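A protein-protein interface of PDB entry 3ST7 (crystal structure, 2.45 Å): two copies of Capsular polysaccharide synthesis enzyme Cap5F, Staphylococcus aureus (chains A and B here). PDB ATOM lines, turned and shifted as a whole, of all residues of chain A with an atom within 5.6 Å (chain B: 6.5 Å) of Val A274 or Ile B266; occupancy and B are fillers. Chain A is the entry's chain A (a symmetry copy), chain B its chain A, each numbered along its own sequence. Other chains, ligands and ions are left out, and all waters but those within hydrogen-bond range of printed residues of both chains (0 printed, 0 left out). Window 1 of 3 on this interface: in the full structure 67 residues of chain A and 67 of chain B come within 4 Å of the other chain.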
ATOM      1  N   THR A 263     -18.471  -0.942   7.148  1.00  0.00           N
ATOM      2  CA  THR A 263     -19.327  -0.413   6.087  1.00  0.00           C
ATOM      3  C   THR A 263     -20.815  -0.616   6.380  1.00  0.00           C
ATOM      4  O   THR A 263     -21.250  -1.746   6.595  1.00  0.00           O
ATOM      5  CB  THR A 263     -19.017  -1.142   4.785  1.00  0.00           C
ATOM      6  OG1 THR A 263     -17.623  -1.040   4.521  1.00  0.00           O
ATOM      7  CG2 THR A 263     -19.789  -0.555   3.633  1.00  0.00           C
ATOM      8  N   GLU A 264     -21.587   0.471   6.371  1.00  0.00           N
ATOM      9  CA  GLU A 264     -23.037   0.405   6.541  1.00  0.00           C
ATOM     10  C   GLU A 264     -23.738  -0.059   5.273  1.00  0.00           C
ATOM     11  O   GLU A 264     -23.399   0.370   4.178  1.00  0.00           O
ATOM     12  CB  GLU A 264     -23.606   1.769   6.954  1.00  0.00           C
ATOM     13  CG  GLU A 264     -23.164   2.204   8.325  1.00  0.00           C
ATOM     14  CD  GLU A 264     -23.604   3.610   8.686  1.00  0.00           C
ATOM     15  OE1 GLU A 264     -23.778   4.453   7.768  1.00  0.00           O
ATOM     16  OE2 GLU A 264     -23.749   3.865   9.908  1.00  0.00           O
ATOM     17  N   PHE A 265     -24.729  -0.921   5.444  1.00  0.00           N
ATOM     18  CA  PHE A 265     -25.473  -1.513   4.347  1.00  0.00           C
ATOM     19  C   PHE A 265     -26.904  -0.963   4.276  1.00  0.00           C
ATOM     20  O   PHE A 265     -27.251  -0.327   3.301  1.00  0.00           O
ATOM     21  CB  PHE A 265     -25.458  -3.041   4.483  1.00  0.00           C
ATOM     22  CG  PHE A 265     -26.290  -3.763   3.464  1.00  0.00           C
ATOM     23  CD1 PHE A 265     -26.431  -3.274   2.163  1.00  0.00           C
ATOM     24  CD2 PHE A 265     -26.906  -4.978   3.794  1.00  0.00           C
ATOM     25  CE1 PHE A 265     -27.221  -3.980   1.206  1.00  0.00           C
ATOM     26  CE2 PHE A 265     -27.703  -5.683   2.855  1.00  0.00           C
ATOM     27  CZ  PHE A 265     -27.833  -5.189   1.556  1.00  0.00           C
ATOM     28  N   ILE A 266     -27.721  -1.216   5.301  1.00  0.00           N
ATOM     29  CA  ILE A 266     -29.089  -0.728   5.375  1.00  0.00           C
ATOM     30  C   ILE A 266     -29.376  -0.127   6.750  1.00  0.00           C
ATOM     31  O   ILE A 266     -28.862  -0.609   7.750  1.00  0.00           O
ATOM     32  CB  ILE A 266     -30.138  -1.814   5.008  1.00  0.00           C
ATOM     33  CG1 ILE A 266     -29.984  -3.059   5.874  1.00  0.00           C
ATOM     34  CG2 ILE A 266     -30.023  -2.214   3.518  1.00  0.00           C
ATOM     35  CD1 ILE A 266     -30.877  -4.264   5.448  1.00  0.00           C
ATOM     36  N   LYS A 267     -30.185   0.935   6.784  1.00  0.00           N
ATOM     37  CA  LYS A 267     -30.477   1.678   8.016  1.00  0.00           C
ATOM     38  C   LYS A 267     -31.987   1.878   8.123  1.00  0.00           C
ATOM     39  O   LYS A 267     -32.608   2.296   7.164  1.00  0.00           O
ATOM     40  CB  LYS A 267     -29.783   3.053   8.001  1.00  0.00           C
ATOM     41  CG  LYS A 267     -28.269   2.959   7.949  1.00  0.00           C
ATOM     42  CD  LYS A 267     -27.541   4.130   8.615  1.00  0.00           C
ATOM     43  CE  LYS A 267     -27.058   5.104   7.591  1.00  0.00           C
ATOM     44  NZ  LYS A 267     -25.967   5.912   8.122  1.00  0.00           N
ATOM     45  N   GLY A 272     -33.634  -1.303  13.357  1.00  0.00           N
ATOM     46  CA  GLY A 272     -32.191  -1.362  13.494  1.00  0.00           C
ATOM     47  C   GLY A 272     -31.497  -1.213  12.163  1.00  0.00           C
ATOM     48  O   GLY A 272     -32.096  -0.754  11.184  1.00  0.00           O
ATOM     49  N   GLN A 273     -30.230  -1.577  12.118  1.00  0.00           N
ATOM     50  CA  GLN A 273     -29.457  -1.386  10.922  1.00  0.00           C
ATOM     51  C   GLN A 273     -28.457  -2.511  10.741  1.00  0.00           C
ATOM     52  O   GLN A 273     -28.118  -3.196  11.708  1.00  0.00           O
ATOM     53  CB  GLN A 273     -28.790  -0.014  10.928  1.00  0.00           C
ATOM     54  CG  GLN A 273     -27.604   0.146  11.783  1.00  0.00           C
ATOM     55  CD  GLN A 273     -26.961   1.554  11.643  1.00  0.00           C
ATOM     56  OE1 GLN A 273     -25.715   1.712  11.581  1.00  0.00           O
ATOM     57  NE2 GLN A 273     -27.816   2.574  11.596  1.00  0.00           N
ATOM     58  N   VAL A 274     -28.026  -2.752   9.504  1.00  0.00           N
ATOM     59  CA  VAL A 274     -27.002  -3.753   9.294  1.00  0.00           C
ATOM     60  C   VAL A 274     -25.774  -3.258   8.569  1.00  0.00           C
ATOM     61  O   VAL A 274     -25.865  -2.478   7.622  1.00  0.00           O
ATOM     62  CB  VAL A 274     -27.548  -5.143   8.789  1.00  0.00           C
ATOM     63  CG1 VAL A 274     -29.041  -5.148   8.620  1.00  0.00           C
ATOM     64  CG2 VAL A 274     -26.767  -5.686   7.613  1.00  0.00           C
ATOM     65  N   SER A 275     -24.621  -3.701   9.071  1.00  0.00           N
ATOM     66  CA  SER A 275     -23.330  -3.287   8.568  1.00  0.00           C
ATOM     67  C   SER A 275     -22.410  -4.477   8.368  1.00  0.00           C
ATOM     68  O   SER A 275     -22.693  -5.595   8.827  1.00  0.00           O
ATOM     69  CB  SER A 275     -22.702  -2.317   9.554  1.00  0.00           C
ATOM     70  OG  SER A 275     -23.581  -1.238   9.821  1.00  0.00           O
ATOM     71  N   VAL A 276     -21.293  -4.233   7.698  1.00  0.00           N
ATOM     72  CA  VAL A 276     -20.343  -5.282   7.431  1.00  0.00           C
ATOM     73  C   VAL A 276     -19.008  -4.883   8.019  1.00  0.00           C
ATOM     74  O   VAL A 276     -18.445  -3.832   7.656  1.00  0.00           O
ATOM     75  CB  VAL A 276     -20.189  -5.506   5.903  1.00  0.00           C
ATOM     76  CG1 VAL A 276     -19.166  -6.593   5.603  1.00  0.00           C
ATOM     77  CG2 VAL A 276     -21.535  -5.826   5.269  1.00  0.00           C
ATOM     78  N   LYS A 296     -26.352  -8.072  16.983  1.00  0.00           N
ATOM     79  CA  LYS A 296     -26.284  -9.472  16.614  1.00  0.00           C
ATOM     80  C   LYS A 296     -25.070  -9.626  15.699  1.00  0.00           C
ATOM     81  O   LYS A 296     -25.017  -8.970  14.678  1.00  0.00           O
ATOM     82  CB  LYS A 296     -27.559  -9.894  15.892  1.00  0.00           C
ATOM     83  CG  LYS A 296     -28.759 -10.076  16.812  1.00  0.00           C
ATOM     84  CD  LYS A 296     -30.050 -10.197  16.006  1.00  0.00           C
ATOM     85  CE  LYS A 296     -31.278 -10.277  16.890  1.00  0.00           C
ATOM     86  NZ  LYS A 296     -31.268 -11.497  17.739  1.00  0.00           N
ATOM     87  N   ILE A 350     -21.200  -9.831   9.755  1.00  0.00           N
ATOM     88  CA  ILE A 350     -22.371  -9.014   9.562  1.00  0.00           C
ATOM     89  C   ILE A 350     -22.863  -8.655  10.948  1.00  0.00           C
ATOM     90  O   ILE A 350     -22.977  -9.530  11.824  1.00  0.00           O
ATOM     91  CB  ILE A 350     -23.468  -9.769   8.789  1.00  0.00           C
ATOM     92  CG1 ILE A 350     -22.914 -10.391   7.495  1.00  0.00           C
ATOM     93  CG2 ILE A 350     -24.636  -8.867   8.490  1.00  0.00           C
ATOM     94  CD1 ILE A 350     -22.137  -9.435   6.542  1.00  0.00           C
ATOM     95  N   MET A 351     -23.138  -7.372  11.152  1.00  0.00           N
ATOM     96  CA  MET A 351     -23.574  -6.868  12.446  1.00  0.00           C
ATOM     97  C   MET A 351     -24.875  -6.120  12.293  1.00  0.00           C
ATOM     98  O   MET A 351     -24.952  -5.151  11.553  1.00  0.00           O
ATOM     99  CB  MET A 351     -22.502  -5.959  13.049  1.00  0.00           C
ATOM    100  CG  MET A 351     -21.111  -6.593  13.049  1.00  0.00           C
ATOM    101  SD  MET A 351     -19.783  -5.538  14.023  1.00  0.00           S
ATOM    102  CE  MET A 351     -18.321  -6.859  14.277  1.00  0.00           C
ATOM    103  N   TRP A 352     -25.917  -6.616  12.950  1.00  0.00           N
ATOM    104  CA  TRP A 352     -27.149  -5.883  13.122  1.00  0.00           C
ATOM    105  C   TRP A 352     -27.002  -5.143  14.446  1.00  0.00           C
ATOM    106  O   TRP A 352     -26.460  -5.695  15.399  1.00  0.00           O
ATOM    107  CB  TRP A 352     -28.348  -6.841  13.181  1.00  0.00           C
ATOM    108  CG  TRP A 352     -29.643  -6.127  13.498  1.00  0.00           C
ATOM    109  CD1 TRP A 352     -30.451  -5.468  12.614  1.00  0.00           C
ATOM    110  CD2 TRP A 352     -30.248  -5.962  14.799  1.00  0.00           C
ATOM    111  NE1 TRP A 352     -31.536  -4.920  13.276  1.00  0.00           N
ATOM    112  CE2 TRP A 352     -31.432  -5.208  14.617  1.00  0.00           C
ATOM    113  CE3 TRP A 352     -29.909  -6.379  16.085  1.00  0.00           C
ATOM    114  CZ2 TRP A 352     -32.278  -4.869  15.679  1.00  0.00           C
ATOM    115  CZ3 TRP A 352     -30.759  -6.038  17.144  1.00  0.00           C
ATOM    116  CH2 TRP A 352     -31.930  -5.292  16.925  1.00  0.00           C
ATOM    117  N   VAL A 353     -27.466  -3.897  14.496  1.00  0.00           N
ATOM    118  CA  VAL A 353     -27.454  -3.097  15.714  1.00  0.00           C
ATOM    119  C   VAL A 353     -28.851  -2.484  15.899  1.00  0.00           C
ATOM    120  O   VAL A 353     -29.534  -2.230  14.914  1.00  0.00           O
ATOM    121  CB  VAL A 353     -26.313  -2.044  15.700  1.00  0.00           C
ATOM    122  CG1 VAL A 353     -26.524  -1.054  14.611  1.00  0.00           C
ATOM    123  CG2 VAL A 353     -26.222  -1.317  17.027  1.00  0.00           C
ATOM    124  N   ASP B 221     -37.828 -17.276  15.135  1.00  0.00           N
ATOM    125  CA  ASP B 221     -38.443 -16.844  13.908  1.00  0.00           C
ATOM    126  C   ASP B 221     -37.728 -15.727  13.165  1.00  0.00           C
ATOM    127  O   ASP B 221     -38.171 -15.278  12.117  1.00  0.00           O
ATOM    128  CB  ASP B 221     -39.984 -16.783  13.963  1.00  0.00           C
ATOM    129  CG  ASP B 221     -40.503 -15.815  14.968  1.00  0.00           C
ATOM    130  OD1 ASP B 221     -39.910 -14.711  15.060  1.00  0.00           O
ATOM    131  OD2 ASP B 221     -41.525 -16.159  15.649  1.00  0.00           O
ATOM    132  N   ARG B 222     -36.557 -15.366  13.700  1.00  0.00           N
ATOM    133  CA  ARG B 222     -35.611 -14.409  13.103  1.00  0.00           C
ATOM    134  C   ARG B 222     -36.146 -12.975  13.102  1.00  0.00           C
ATOM    135  O   ARG B 222     -35.628 -12.118  12.398  1.00  0.00           O
ATOM    136  CB  ARG B 222     -35.207 -14.810  11.671  1.00  0.00           C
ATOM    137  CG  ARG B 222     -34.846 -16.296  11.418  1.00  0.00           C
ATOM    138  CD  ARG B 222     -33.855 -16.828  12.451  1.00  0.00           C
ATOM    139  NE  ARG B 222     -33.600 -18.233  12.202  1.00  0.00           N
ATOM    140  CZ  ARG B 222     -33.227 -19.124  13.118  1.00  0.00           C
ATOM    141  NH1 ARG B 222     -33.075 -18.773  14.386  1.00  0.00           N
ATOM    142  NH2 ARG B 222     -33.027 -20.387  12.755  1.00  0.00           N
ATOM    143  N   THR B 223     -37.199 -12.725  13.863  1.00  0.00           N
ATOM    144  CA  THR B 223     -37.817 -11.415  13.870  1.00  0.00           C
ATOM    145  C   THR B 223     -37.132 -10.473  14.860  1.00  0.00           C
ATOM    146  O   THR B 223     -36.228 -10.851  15.619  1.00  0.00           O
ATOM    147  CB  THR B 223     -39.320 -11.496  14.199  1.00  0.00           C
ATOM    148  OG1 THR B 223     -39.488 -12.176  15.442  1.00  0.00           O
ATOM    149  CG2 THR B 223     -40.104 -12.219  13.088  1.00  0.00           C
ATOM    150  N   LEU B 224     -37.596  -9.237  14.857  1.00  0.00           N
ATOM    151  CA  LEU B 224     -36.912  -8.125  15.478  1.00  0.00           C
ATOM    152  C   LEU B 224     -37.936  -7.279  16.231  1.00  0.00           C
ATOM    153  O   LEU B 224     -39.104  -7.192  15.834  1.00  0.00           O
ATOM    154  CB  LEU B 224     -36.283  -7.296  14.370  1.00  0.00           C
ATOM    155  CG  LEU B 224     -34.797  -7.330  14.013  1.00  0.00           C
ATOM    156  CD1 LEU B 224     -34.020  -8.504  14.493  1.00  0.00           C
ATOM    157  CD2 LEU B 224     -34.570  -7.034  12.549  1.00  0.00           C
ATOM    158  N   TYR B 250     -27.199 -18.489  18.899  1.00  0.00           N
ATOM    159  CA  TYR B 250     -28.199 -19.419  18.398  1.00  0.00           C
ATOM    160  C   TYR B 250     -27.876 -19.784  16.953  1.00  0.00           C
ATOM    161  O   TYR B 250     -27.419 -18.939  16.197  1.00  0.00           O
ATOM    162  CB  TYR B 250     -29.634 -18.880  18.551  1.00  0.00           C
ATOM    163  CG  TYR B 250     -29.915 -17.552  17.896  1.00  0.00           C
ATOM    164  CD1 TYR B 250     -29.597 -16.366  18.546  1.00  0.00           C
ATOM    165  CD2 TYR B 250     -30.520 -17.470  16.637  1.00  0.00           C
ATOM    166  CE1 TYR B 250     -29.841 -15.118  17.970  1.00  0.00           C
ATOM    167  CE2 TYR B 250     -30.773 -16.207  16.032  1.00  0.00           C
ATOM    168  CZ  TYR B 250     -30.427 -15.039  16.720  1.00  0.00           C
ATOM    169  OH  TYR B 250     -30.654 -13.789  16.190  1.00  0.00           O
ATOM    170  N   LEU B 252     -28.375 -20.635  13.038  1.00  0.00           N
ATOM    171  CA  LEU B 252     -29.287 -20.277  11.972  1.00  0.00           C
ATOM    172  C   LEU B 252     -29.619 -21.553  11.190  1.00  0.00           C
ATOM    173  O   LEU B 252     -28.958 -22.574  11.360  1.00  0.00           O
ATOM    174  CB  LEU B 252     -28.624 -19.243  11.087  1.00  0.00           C
ATOM    175  CG  LEU B 252     -29.030 -17.763  11.199  1.00  0.00           C
ATOM    176  CD1 LEU B 252     -29.881 -17.340  12.404  1.00  0.00           C
ATOM    177  CD2 LEU B 252     -27.824 -16.885  11.028  1.00  0.00           C
ATOM    178  N   GLU B 264     -31.349 -17.654   6.227  1.00  0.00           N
ATOM    179  CA  GLU B 264     -32.025 -16.448   6.702  1.00  0.00           C
ATOM    180  C   GLU B 264     -31.422 -15.932   7.999  1.00  0.00           C
ATOM    181  O   GLU B 264     -31.122 -16.703   8.900  1.00  0.00           O
ATOM    182  CB  GLU B 264     -33.522 -16.704   6.915  1.00  0.00           C
ATOM    183  CG  GLU B 264     -34.265 -16.977   5.636  1.00  0.00           C
ATOM    184  CD  GLU B 264     -35.714 -17.370   5.848  1.00  0.00           C
ATOM    185  OE1 GLU B 264     -36.044 -17.943   6.918  1.00  0.00           O
ATOM    186  OE2 GLU B 264     -36.514 -17.119   4.913  1.00  0.00           O
ATOM    187  N   PHE B 265     -31.272 -14.618   8.084  1.00  0.00           N
ATOM    188  CA  PHE B 265     -30.664 -13.953   9.222  1.00  0.00           C
ATOM    189  C   PHE B 265     -31.705 -13.178  10.042  1.00  0.00           C
ATOM    190  O   PHE B 265     -31.926 -13.510  11.190  1.00  0.00           O
ATOM    191  CB  PHE B 265     -29.530 -13.041   8.737  1.00  0.00           C
ATOM    192  CG  PHE B 265     -28.895 -12.214   9.816  1.00  0.00           C
ATOM    193  CD1 PHE B 265     -28.766 -12.696  11.120  1.00  0.00           C
ATOM    194  CD2 PHE B 265     -28.372 -10.948   9.515  1.00  0.00           C
ATOM    195  CE1 PHE B 265     -28.151 -11.896  12.131  1.00  0.00           C
ATOM    196  CE2 PHE B 265     -27.770 -10.140  10.513  1.00  0.00           C
ATOM    197  CZ  PHE B 265     -27.641 -10.633  11.812  1.00  0.00           C
ATOM    198  N   ILE B 266     -32.326 -12.154   9.454  1.00  0.00           N
ATOM    199  CA  ILE B 266     -33.353 -11.358  10.107  1.00  0.00           C
ATOM    200  C   ILE B 266     -34.554 -11.161   9.183  1.00  0.00           C
ATOM    201  O   ILE B 266     -34.388 -11.043   7.976  1.00  0.00           O
ATOM    202  CB  ILE B 266     -32.819  -9.995  10.629  1.00  0.00           C
ATOM    203  CG1 ILE B 266     -32.164  -9.185   9.518  1.00  0.00           C
ATOM    204  CG2 ILE B 266     -31.801 -10.203  11.776  1.00  0.00           C
ATOM    205  CD1 ILE B 266     -31.441  -7.888   9.996  1.00  0.00           C
ATOM    206  N   LYS B 267     -35.759 -11.143   9.759  1.00  0.00           N
ATOM    207  CA  LYS B 267     -37.009 -11.059   8.995  1.00  0.00           C
ATOM    208  C   LYS B 267     -37.891  -9.977   9.614  1.00  0.00           C
ATOM    209  O   LYS B 267     -38.073  -9.964  10.816  1.00  0.00           O
ATOM    210  CB  LYS B 267     -37.760 -12.404   9.027  1.00  0.00           C
ATOM    211  CG  LYS B 267     -36.982 -13.539   8.385  1.00  0.00           C
ATOM    212  CD  LYS B 267     -37.858 -14.631   7.763  1.00  0.00           C
ATOM    213  CE  LYS B 267     -37.947 -15.815   8.668  1.00  0.00           C
ATOM    214  NZ  LYS B 267     -38.318 -17.009   7.918  1.00  0.00           N
ATOM    215  N   THR B 268     -38.453  -9.078   8.821  1.00  0.00           N
ATOM    216  CA  THR B 268     -39.360  -8.093   9.371  1.00  0.00           C
ATOM    217  C   THR B 268     -40.620  -8.022   8.536  1.00  0.00           C
ATOM    218  O   THR B 268     -40.587  -8.296   7.355  1.00  0.00           O
ATOM    219  CB  THR B 268     -38.719  -6.663   9.408  1.00  0.00           C
ATOM    220  OG1 THR B 268     -38.687  -6.132   8.079  1.00  0.00           O
ATOM    221  CG2 THR B 268     -37.310  -6.705   9.941  1.00  0.00           C
ATOM    222  N   GLY B 272     -38.461  -5.608   5.052  1.00  0.00           N
ATOM    223  CA  GLY B 272     -37.826  -6.662   4.285  1.00  0.00           C
ATOM    224  C   GLY B 272     -37.045  -7.602   5.169  1.00  0.00           C
ATOM    225  O   GLY B 272     -37.240  -7.635   6.388  1.00  0.00           O
ATOM    226  N   GLN B 273     -36.172  -8.386   4.564  1.00  0.00           N
ATOM    227  CA  GLN B 273     -35.446  -9.380   5.306  1.00  0.00           C
ATOM    228  C   GLN B 273     -34.043  -9.543   4.758  1.00  0.00           C
ATOM    229  O   GLN B 273     -33.783  -9.180   3.609  1.00  0.00           O
ATOM    230  CB  GLN B 273     -36.216 -10.698   5.331  1.00  0.00           C
ATOM    231  CG  GLN B 273     -36.182 -11.511   4.106  1.00  0.00           C
ATOM    232  CD  GLN B 273     -36.926 -12.865   4.276  1.00  0.00           C
ATOM    233  OE1 GLN B 273     -36.462 -13.940   3.820  1.00  0.00           O
ATOM    234  NE2 GLN B 273     -38.083 -12.806   4.934  1.00  0.00           N
ATOM    235  N   VAL B 274     -33.117 -10.030   5.584  1.00  0.00           N
ATOM    236  CA  VAL B 274     -31.786 -10.292   5.079  1.00  0.00           C
ATOM    237  C   VAL B 274     -31.300 -11.706   5.284  1.00  0.00           C
ATOM    238  O   VAL B 274     -31.530 -12.313   6.329  1.00  0.00           O
ATOM    239  CB  VAL B 274     -30.729  -9.176   5.429  1.00  0.00           C
ATOM    240  CG1 VAL B 274     -31.322  -8.052   6.231  1.00  0.00           C
ATOM    241  CG2 VAL B 274     -29.439  -9.743   5.977  1.00  0.00           C
ATOM    242  N   SER B 275     -30.658 -12.226   4.238  1.00  0.00           N
ATOM    243  CA  SER B 275     -30.177 -13.589   4.204  1.00  0.00           C
ATOM    244  C   SER B 275     -28.751 -13.657   3.692  1.00  0.00           C
ATOM    245  O   SER B 275     -28.211 -12.677   3.155  1.00  0.00           O
ATOM    246  CB  SER B 275     -31.083 -14.411   3.302  1.00  0.00           C
ATOM    247  OG  SER B 275     -32.434 -14.294   3.711  1.00  0.00           O
ATOM    248  N   ILE B 350     -24.654 -11.149   0.695  1.00  0.00           N
ATOM    249  CA  ILE B 350     -25.731 -10.760   1.570  1.00  0.00           C
ATOM    250  C   ILE B 350     -26.841 -10.260   0.670  1.00  0.00           C
ATOM    251  O   ILE B 350     -26.597  -9.455  -0.245  1.00  0.00           O
ATOM    252  CB  ILE B 350     -25.298  -9.650   2.545  1.00  0.00           C
ATOM    253  CG1 ILE B 350     -23.996 -10.023   3.275  1.00  0.00           C
ATOM    254  CG2 ILE B 350     -26.393  -9.338   3.529  1.00  0.00           C
ATOM    255  CD1 ILE B 350     -23.970 -11.409   3.985  1.00  0.00           C
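The side-chain amino group (NZ) of Lys A296 lies within hydrogen-bond range of the side-chain hydroxyl (OH) of Tyr B250 (2.8 Å).
N of Phe B265 sits at hydrogen-bond distance from O of Val B274, 2.9 Å away. O of Ile B266 sits at hydrogen-bond distance from N of Val B274 (2.9 Å). The backbone NH of Phe A265 is in hydrogen-bond range of the backbone carbonyl oxygen of Val A274 (2.9 Å). The backbone NH of Val A274 is in hydrogen-bond range of the backbone carbonyl oxygen of Ile A266, 2.9 Å away. The backbone NH (N) of Lys A296 lies within hydrogen-bond range of the backbone carbonyl oxygen (O) of Trp A352, at 2.9 Å.
Among the printed residues, merely in contact across the chains: Phe A265 with Ile B350, Ile A266 with Val B274, Val A274 with Ile B266, Ile A350 with Phe B265, Ile A350 with Ile B350, Trp A352 with Leu B224 and Trp A352 with Ile B266.
Val A274 touches just one residue of chain B: Ile B266. Of the printed residues of chain B, Lys A296 touches Tyr B250 (2.8 Å). Printed residues of chain B within 4 Å of Ile A350: Phe B265 (3.9 Å) and Ile B350 (3.7 Å). Of the printed residues of chain B, Trp A352 touches Leu B224 and Ile B266. Of the printed residues of chain A, Tyr B250 touches Lys A296 (2.8 Å). Ile B266 touches two residues of chain A. Lys B267 touches none of the printed residues of chain A. Gly B272 touches none of the printed residues of chain A. Printed residues of chain A within 4 Å of Ile B350: Phe A265 (3.9 Å) and Ile A350 (3.7 Å). The nearest residue of chain B that does not touch Val A274 is Val B274 (4.4 Å). The nearest residue of chain A that does not touch Ile B266 is Lys A296 (4.6 Å). The nearest printed residue of chain B that does not touch Lys A296 is Leu B224 (4.1 Å).
Hydrophobic or aromatic side chains of chain B within 4 Å of the printed part of chain A: Leu B224, Tyr B250, Phe B265, Ile B266, Val B274 and Ile B350. Printed residues of chain A that touch a printed residue of chain B: Phe A265, Ile A266, Val A274, Lys A296, Ile A350 and Trp A352. Hydrophobic or aromatic side chains of chain A within 4 Å of the printed part of chain B: Phe A265, Ile A266, Val A274, Ile A350 and Trp A352. Among the printed residues, 8 pairs touch across the chains.
Phe A265 touches Ile B350, and with the chains exchanged Ile A350 touches Phe B265. Ile A266 touches Val B274, and with the chains exchanged Val A274 touches Ile B266. Ile B350 touches its own counterpart, Ile A350. Of the 8 pairs that touch across the chains among the printed residues, 5 have their exchanged pair printed and touching as well.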
